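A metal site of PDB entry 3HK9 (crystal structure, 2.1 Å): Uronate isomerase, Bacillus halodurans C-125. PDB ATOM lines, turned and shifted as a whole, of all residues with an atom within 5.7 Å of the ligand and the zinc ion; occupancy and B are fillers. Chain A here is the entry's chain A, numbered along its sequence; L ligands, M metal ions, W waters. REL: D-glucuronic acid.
Residues that only touch the ligand: Met 258, Trp 326 and Ser 223. Hydrophobic or aromatic side chains that line the ligand: His 26, His 28, His 49, Tyr 50, Met 258, Trp 325 and Trp 326. 11 residues have an atom within 4 Å of the ligand: His 26, His 28, His 49, Tyr 50, Arg 170, Ser 223, Met 258, Trp 325, Trp 326, Asp 355 and Arg 357.
Three residues have an atom within 4 Å of the zinc ion: His 26, His 28 and Asp 355.
A ring nitrogen (ND1) of His 26 sits close to the side-chain hydroxyl (OG1) of Thr 143 (3.4 Å). NE1 of Trp 325 sits close to OD2 of Asp 355 (3.2 Å). OD2 of Asp 355 is in hydrogen-bond range of NE2 of His 353. The guanidinium group of Arg 170 lies close to the side-chain hydroxyl of Ser 223, 3.3 Å away. OD1 of Asp 172 is in salt-bridge range of NE of Arg 170 (2.6 Å). ND1 of His 49 is in hydrogen-bond range of O of Asp 271. The side-chain hydroxyl of Ser 223 sits at hydrogen-bond distance from the side-chain carboxylate of Asp 172.
An oxygen (O1) of the ligand is in hydrogen-bond range of the side-chain hydroxyl (OH) of Tyr 50. NE of Arg 357 is in hydrogen-bond range of O2 of the ligand, 2.6 Å away. The guanidinium group (NH2) of Arg 170 lies within salt-bridge range of an oxygen (O6A) of the ligand, at 2.7 Å. The indole nitrogen (NE1) of Trp 325 sits close to an oxygen (O5) of the ligand (2.8 Å). NE2 of His 49 sits at hydrogen-bond distance from O3 of the ligand, 2.9 Å away.
Water W2 lies within hydrogen-bond range of OD2 of Asp 274 (2.6 Å), O of Asp 271 (2.8 Å) and O3 of the ligand (2.8 Å). Water W1 lies within hydrogen-bond range of O6A of the ligand, NZ of Lys 263 and OG of Ser 223.
The zinc ion is bound by O5 of the ligand (2.0 Å), NE2 of His 28 (2.2 Å), NE2 of His 26 (2.2 Å), OD1 of Asp 355 (2.2 Å) and O6B of the ligand (2.3 Å). The zinc ion has five donor atoms within binding distance.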
ATOM      1  N   HIS A  26      -4.998 -19.259 -12.735  1.00  0.00           N
ATOM      2  CA  HIS A  26      -3.893 -19.294 -11.779  1.00  0.00           C
ATOM      3  C   HIS A  26      -3.467 -17.883 -11.385  1.00  0.00           C
ATOM      4  O   HIS A  26      -2.954 -17.125 -12.204  1.00  0.00           O
ATOM      5  CB  HIS A  26      -2.647 -20.046 -12.273  1.00  0.00           C
ATOM      6  CG  HIS A  26      -1.505 -20.013 -11.294  1.00  0.00           C
ATOM      7  ND1 HIS A  26      -1.639 -20.423  -9.982  1.00  0.00           N
ATOM      8  CD2 HIS A  26      -0.229 -19.558 -11.407  1.00  0.00           C
ATOM      9  CE1 HIS A  26      -0.500 -20.228  -9.337  1.00  0.00           C
ATOM     10  NE2 HIS A  26       0.372 -19.704 -10.181  1.00  0.00           N
ATOM     11  N   THR A  27      -3.697 -17.564 -10.116  1.00  0.00           N
ATOM     12  CA  THR A  27      -3.357 -16.253  -9.565  1.00  0.00           C
ATOM     13  C   THR A  27      -2.984 -16.439  -8.102  1.00  0.00           C
ATOM     14  O   THR A  27      -3.160 -17.517  -7.533  1.00  0.00           O
ATOM     15  CB  THR A  27      -4.561 -15.299  -9.591  1.00  0.00           C
ATOM     16  OG1 THR A  27      -5.476 -15.657  -8.550  1.00  0.00           O
ATOM     17  CG2 THR A  27      -5.286 -15.367 -10.930  1.00  0.00           C
ATOM     18  N   HIS A  28      -2.486 -15.363  -7.491  1.00  0.00           N
ATOM     19  CA  HIS A  28      -2.136 -15.381  -6.080  1.00  0.00           C
ATOM     20  C   HIS A  28      -3.011 -14.331  -5.410  1.00  0.00           C
ATOM     21  O   HIS A  28      -2.579 -13.627  -4.487  1.00  0.00           O
ATOM     22  CB  HIS A  28      -0.657 -15.073  -5.904  1.00  0.00           C
ATOM     23  CG  HIS A  28       0.235 -16.159  -6.415  1.00  0.00           C
ATOM     24  ND1 HIS A  28       0.464 -17.317  -5.722  1.00  0.00           N
ATOM     25  CD2 HIS A  28       0.879 -16.297  -7.606  1.00  0.00           C
ATOM     26  CE1 HIS A  28       1.211 -18.126  -6.449  1.00  0.00           C
ATOM     27  NE2 HIS A  28       1.476 -17.527  -7.595  1.00  0.00           N
ATOM     28  N   TYR A  48       6.021  -5.440  -6.129  1.00  0.00           N
ATOM     29  CA  TYR A  48       5.839  -6.779  -6.694  1.00  0.00           C
ATOM     30  C   TYR A  48       7.283  -7.299  -6.724  1.00  0.00           C
ATOM     31  O   TYR A  48       8.203  -6.541  -7.036  1.00  0.00           O
ATOM     32  CB  TYR A  48       5.258  -6.631  -8.098  1.00  0.00           C
ATOM     33  CG  TYR A  48       5.030  -7.878  -8.911  1.00  0.00           C
ATOM     34  CD1 TYR A  48       4.498  -9.033  -8.346  1.00  0.00           C
ATOM     35  CD2 TYR A  48       5.250  -7.868 -10.287  1.00  0.00           C
ATOM     36  CE1 TYR A  48       4.161 -10.149  -9.155  1.00  0.00           C
ATOM     37  CE2 TYR A  48       4.925  -8.962 -11.095  1.00  0.00           C
ATOM     38  CZ  TYR A  48       4.381 -10.091 -10.524  1.00  0.00           C
ATOM     39  OH  TYR A  48       4.008 -11.135 -11.338  1.00  0.00           O
ATOM     40  N   HIS A  49       7.505  -8.578  -6.425  1.00  0.00           N
ATOM     41  CA  HIS A  49       8.883  -9.062  -6.393  1.00  0.00           C
ATOM     42  C   HIS A  49       9.649  -8.957  -7.708  1.00  0.00           C
ATOM     43  O   HIS A  49      10.890  -8.919  -7.702  1.00  0.00           O
ATOM     44  CB  HIS A  49       8.967 -10.471  -5.770  1.00  0.00           C
ATOM     45  CG  HIS A  49       8.490 -11.590  -6.638  1.00  0.00           C
ATOM     46  ND1 HIS A  49       9.255 -12.146  -7.634  1.00  0.00           N
ATOM     47  CD2 HIS A  49       7.364 -12.345  -6.582  1.00  0.00           C
ATOM     48  CE1 HIS A  49       8.635 -13.197  -8.150  1.00  0.00           C
ATOM     49  NE2 HIS A  49       7.488 -13.338  -7.520  1.00  0.00           N
ATOM     50  N   TYR A  50       8.935  -8.871  -8.831  1.00  0.00           N
ATOM     51  CA  TYR A  50       9.596  -8.730 -10.127  1.00  0.00           C
ATOM     52  C   TYR A  50      10.380  -7.424 -10.119  1.00  0.00           C
ATOM     53  O   TYR A  50      11.494  -7.346 -10.642  1.00  0.00           O
ATOM     54  CB  TYR A  50       8.560  -8.659 -11.274  1.00  0.00           C
ATOM     55  CG  TYR A  50       7.957  -9.975 -11.713  1.00  0.00           C
ATOM     56  CD1 TYR A  50       7.666 -10.995 -10.794  1.00  0.00           C
ATOM     57  CD2 TYR A  50       7.619 -10.189 -13.056  1.00  0.00           C
ATOM     58  CE1 TYR A  50       7.038 -12.184 -11.211  1.00  0.00           C
ATOM     59  CE2 TYR A  50       6.999 -11.374 -13.474  1.00  0.00           C
ATOM     60  CZ  TYR A  50       6.715 -12.361 -12.552  1.00  0.00           C
ATOM     61  OH  TYR A  50       6.113 -13.537 -12.972  1.00  0.00           O
ATOM     62  N   THR A 143      -4.511 -19.608  -5.259  1.00  0.00           N
ATOM     63  CA  THR A 143      -3.536 -20.622  -4.911  1.00  0.00           C
ATOM     64  C   THR A 143      -3.717 -20.722  -3.410  1.00  0.00           C
ATOM     65  O   THR A 143      -3.289 -19.830  -2.657  1.00  0.00           O
ATOM     66  CB  THR A 143      -2.087 -20.184  -5.221  1.00  0.00           C
ATOM     67  OG1 THR A 143      -1.912 -20.044  -6.629  1.00  0.00           O
ATOM     68  CG2 THR A 143      -1.106 -21.228  -4.696  1.00  0.00           C
ATOM     69  N   ARG A 170      -2.947 -26.103  -3.300  1.00  0.00           N
ATOM     70  CA  ARG A 170      -1.498 -26.093  -3.515  1.00  0.00           C
ATOM     71  C   ARG A 170      -0.832 -27.049  -2.513  1.00  0.00           C
ATOM     72  O   ARG A 170      -1.069 -26.958  -1.302  1.00  0.00           O
ATOM     73  CB  ARG A 170      -0.992 -24.662  -3.361  1.00  0.00           C
ATOM     74  CG  ARG A 170       0.424 -24.437  -3.853  1.00  0.00           C
ATOM     75  CD  ARG A 170       0.620 -24.898  -5.302  1.00  0.00           C
ATOM     76  NE  ARG A 170       2.008 -24.678  -5.688  1.00  0.00           N
ATOM     77  CZ  ARG A 170       2.467 -23.557  -6.257  1.00  0.00           C
ATOM     78  NH1 ARG A 170       1.641 -22.553  -6.535  1.00  0.00           N
ATOM     79  NH2 ARG A 170       3.763 -23.424  -6.482  1.00  0.00           N
ATOM     80  N   ASP A 172       2.884 -27.982  -2.445  1.00  0.00           N
ATOM     81  CA  ASP A 172       4.351 -27.996  -2.449  1.00  0.00           C
ATOM     82  C   ASP A 172       5.013 -28.599  -1.195  1.00  0.00           C
ATOM     83  O   ASP A 172       5.923 -29.426  -1.303  1.00  0.00           O
ATOM     84  CB  ASP A 172       4.900 -26.581  -2.698  1.00  0.00           C
ATOM     85  CG  ASP A 172       4.562 -26.059  -4.095  1.00  0.00           C
ATOM     86  OD1 ASP A 172       3.577 -26.553  -4.688  1.00  0.00           O
ATOM     87  OD2 ASP A 172       5.252 -25.140  -4.601  1.00  0.00           O
ATOM     88  N   SER A 223       4.512 -26.877  -7.609  1.00  0.00           N
ATOM     89  CA  SER A 223       5.550 -26.333  -8.484  1.00  0.00           C
ATOM     90  C   SER A 223       6.696 -27.323  -8.276  1.00  0.00           C
ATOM     91  O   SER A 223       6.915 -27.795  -7.161  1.00  0.00           O
ATOM     92  CB  SER A 223       5.970 -24.909  -8.087  1.00  0.00           C
ATOM     93  OG  SER A 223       6.676 -24.880  -6.859  1.00  0.00           O
ATOM     94  N   MET A 258       3.574 -27.223 -12.298  1.00  0.00           N
ATOM     95  CA  MET A 258       4.267 -26.070 -12.845  1.00  0.00           C
ATOM     96  C   MET A 258       5.744 -26.421 -12.677  1.00  0.00           C
ATOM     97  O   MET A 258       6.309 -26.324 -11.579  1.00  0.00           O
ATOM     98  CB  MET A 258       3.865 -24.829 -12.057  1.00  0.00           C
ATOM     99  CG  MET A 258       2.369 -24.795 -11.783  1.00  0.00           C
ATOM    100  SD  MET A 258       1.686 -23.147 -11.742  1.00  0.00           S
ATOM    101  CE  MET A 258       2.074 -22.676 -10.098  1.00  0.00           C
ATOM    102  N   LYS A 263      14.120 -23.175  -6.668  1.00  0.00           N
ATOM    103  CA  LYS A 263      13.875 -22.368  -5.475  1.00  0.00           C
ATOM    104  C   LYS A 263      15.087 -21.760  -4.783  1.00  0.00           C
ATOM    105  O   LYS A 263      16.137 -22.376  -4.665  1.00  0.00           O
ATOM    106  CB  LYS A 263      13.073 -23.187  -4.453  1.00  0.00           C
ATOM    107  CG  LYS A 263      11.743 -23.709  -4.957  1.00  0.00           C
ATOM    108  CD  LYS A 263      10.804 -22.587  -5.393  1.00  0.00           C
ATOM    109  CE  LYS A 263      10.373 -21.707  -4.233  1.00  0.00           C
ATOM    110  NZ  LYS A 263       9.417 -20.646  -4.681  1.00  0.00           N
ATOM    111  N   ASP A 271      11.076 -13.780  -2.242  1.00  0.00           N
ATOM    112  CA  ASP A 271      10.275 -14.250  -3.371  1.00  0.00           C
ATOM    113  C   ASP A 271      10.901 -13.938  -4.724  1.00  0.00           C
ATOM    114  O   ASP A 271      10.521 -14.501  -5.741  1.00  0.00           O
ATOM    115  CB  ASP A 271       8.871 -13.640  -3.308  1.00  0.00           C
ATOM    116  CG  ASP A 271       7.990 -14.294  -2.262  1.00  0.00           C
ATOM    117  OD1 ASP A 271       8.292 -15.432  -1.858  1.00  0.00           O
ATOM    118  OD2 ASP A 271       6.982 -13.665  -1.862  1.00  0.00           O
ATOM    119  N   ASP A 274      14.095 -16.823  -6.945  1.00  0.00           N
ATOM    120  CA  ASP A 274      13.935 -18.117  -7.595  1.00  0.00           C
ATOM    121  C   ASP A 274      14.505 -18.100  -9.020  1.00  0.00           C
ATOM    122  O   ASP A 274      14.394 -17.097  -9.736  1.00  0.00           O
ATOM    123  CB  ASP A 274      12.451 -18.537  -7.639  1.00  0.00           C
ATOM    124  CG  ASP A 274      11.857 -18.760  -6.230  1.00  0.00           C
ATOM    125  OD1 ASP A 274      12.613 -19.123  -5.305  1.00  0.00           O
ATOM    126  OD2 ASP A 274      10.638 -18.588  -6.067  1.00  0.00           O
ATOM    127  N   TRP A 325       4.155 -18.819 -18.101  1.00  0.00           N
ATOM    128  CA  TRP A 325       4.516 -18.637 -16.709  1.00  0.00           C
ATOM    129  C   TRP A 325       5.807 -17.913 -16.330  1.00  0.00           C
ATOM    130  O   TRP A 325       6.890 -18.241 -16.814  1.00  0.00           O
ATOM    131  CB  TRP A 325       4.513 -20.020 -16.057  1.00  0.00           C
ATOM    132  CG  TRP A 325       4.755 -20.049 -14.574  1.00  0.00           C
ATOM    133  CD1 TRP A 325       4.243 -19.203 -13.635  1.00  0.00           C
ATOM    134  CD2 TRP A 325       5.471 -21.070 -13.846  1.00  0.00           C
ATOM    135  NE1 TRP A 325       4.592 -19.625 -12.373  1.00  0.00           N
ATOM    136  CE2 TRP A 325       5.343 -20.766 -12.476  1.00  0.00           C
ATOM    137  CE3 TRP A 325       6.208 -22.193 -14.228  1.00  0.00           C
ATOM    138  CZ2 TRP A 325       5.929 -21.561 -11.472  1.00  0.00           C
ATOM    139  CZ3 TRP A 325       6.786 -22.992 -13.223  1.00  0.00           C
ATOM    140  CH2 TRP A 325       6.640 -22.660 -11.875  1.00  0.00           C
ATOM    141  N   TRP A 326       5.655 -16.908 -15.465  1.00  0.00           N
ATOM    142  CA  TRP A 326       6.783 -16.204 -14.873  1.00  0.00           C
ATOM    143  C   TRP A 326       7.783 -15.567 -15.851  1.00  0.00           C
ATOM    144  O   TRP A 326       7.532 -14.510 -16.422  1.00  0.00           O
ATOM    145  CB  TRP A 326       7.506 -17.218 -13.992  1.00  0.00           C
ATOM    146  CG  TRP A 326       8.195 -16.724 -12.778  1.00  0.00           C
ATOM    147  CD1 TRP A 326       8.736 -15.487 -12.577  1.00  0.00           C
ATOM    148  CD2 TRP A 326       8.510 -17.496 -11.622  1.00  0.00           C
ATOM    149  NE1 TRP A 326       9.379 -15.445 -11.356  1.00  0.00           N
ATOM    150  CE2 TRP A 326       9.258 -16.673 -10.754  1.00  0.00           C
ATOM    151  CE3 TRP A 326       8.236 -18.815 -11.241  1.00  0.00           C
ATOM    152  CZ2 TRP A 326       9.731 -17.126  -9.521  1.00  0.00           C
ATOM    153  CZ3 TRP A 326       8.706 -19.267 -10.022  1.00  0.00           C
ATOM    154  CH2 TRP A 326       9.450 -18.418  -9.172  1.00  0.00           C
ATOM    155  N   HIS A 353      -2.523 -17.036 -18.191  1.00  0.00           N
ATOM    156  CA  HIS A 353      -3.036 -16.844 -16.830  1.00  0.00           C
ATOM    157  C   HIS A 353      -2.260 -15.618 -16.351  1.00  0.00           C
ATOM    158  O   HIS A 353      -1.200 -15.323 -16.892  1.00  0.00           O
ATOM    159  CB  HIS A 353      -2.805 -18.060 -15.920  1.00  0.00           C
ATOM    160  CG  HIS A 353      -1.367 -18.327 -15.573  1.00  0.00           C
ATOM    161  ND1 HIS A 353      -0.556 -19.119 -16.348  1.00  0.00           N
ATOM    162  CD2 HIS A 353      -0.628 -17.933 -14.514  1.00  0.00           C
ATOM    163  CE1 HIS A 353       0.640 -19.198 -15.780  1.00  0.00           C
ATOM    164  NE2 HIS A 353       0.625 -18.490 -14.663  1.00  0.00           N
ATOM    165  N   ASP A 355      -1.311 -14.854 -12.941  1.00  0.00           N
ATOM    166  CA  ASP A 355      -0.386 -15.152 -11.860  1.00  0.00           C
ATOM    167  C   ASP A 355      -0.354 -13.899 -10.977  1.00  0.00           C
ATOM    168  O   ASP A 355       0.640 -13.627 -10.300  1.00  0.00           O
ATOM    169  CB  ASP A 355       1.023 -15.408 -12.416  1.00  0.00           C
ATOM    170  CG  ASP A 355       1.789 -16.467 -11.630  1.00  0.00           C
ATOM    171  OD1 ASP A 355       1.538 -16.622 -10.420  1.00  0.00           O
ATOM    172  OD2 ASP A 355       2.642 -17.136 -12.236  1.00  0.00           O
ATOM    173  N   ARG A 357      -0.363 -11.246  -8.166  1.00  0.00           N
ATOM    174  CA  ARG A 357      -0.041 -11.272  -6.743  1.00  0.00           C
ATOM    175  C   ARG A 357      -0.658 -10.014  -6.149  1.00  0.00           C
ATOM    176  O   ARG A 357      -0.923  -9.940  -4.956  1.00  0.00           O
ATOM    177  CB  ARG A 357       1.477 -11.263  -6.535  1.00  0.00           C
ATOM    178  CG  ARG A 357       2.137 -12.625  -6.620  1.00  0.00           C
ATOM    179  CD  ARG A 357       3.624 -12.542  -6.382  1.00  0.00           C
ATOM    180  NE  ARG A 357       4.241 -13.848  -6.174  1.00  0.00           N
ATOM    181  CZ  ARG A 357       4.104 -14.585  -5.073  1.00  0.00           C
ATOM    182  NH1 ARG A 357       3.371 -14.136  -4.062  1.00  0.00           N
ATOM    183  NH2 ARG A 357       4.700 -15.764  -4.975  1.00  0.00           N
HETATM  184  O6A REL L   1       4.750 -21.369  -7.944  1.00  0.00           O
HETATM  185  C6  REL L   1       4.035 -20.385  -8.299  1.00  0.00           C
HETATM  186  O6B REL L   1       2.797 -20.336  -8.228  1.00  0.00           O
HETATM  187  C5  REL L   1       4.792 -19.188  -8.875  1.00  0.00           C
HETATM  188  O5  REL L   1       3.961 -18.579  -9.875  1.00  0.00           O
HETATM  189  C4  REL L   1       5.152 -18.113  -7.807  1.00  0.00           C
HETATM  190  O4  REL L   1       6.010 -18.764  -6.847  1.00  0.00           O
HETATM  191  C3  REL L   1       5.882 -16.855  -8.355  1.00  0.00           C
HETATM  192  O3  REL L   1       6.419 -16.048  -7.287  1.00  0.00           O
HETATM  193  C2  REL L   1       4.937 -16.007  -9.242  1.00  0.00           C
HETATM  194  O2  REL L   1       4.464 -14.855  -8.553  1.00  0.00           O
HETATM  195  C1  REL L   1       5.633 -15.595 -10.537  1.00  0.00           C
HETATM  196  O1  REL L   1       4.997 -15.419 -11.585  1.00  0.00           O
HETATM  197 ZN    ZN M   1       2.062 -18.519  -9.414  1.00  0.00          ZN
HETATM  198  O   HOH W   1       7.494 -21.508  -6.879  1.00  0.00           O
HETATM  199  O   HOH W   2       8.839 -16.760  -5.970  1.00  0.00           O
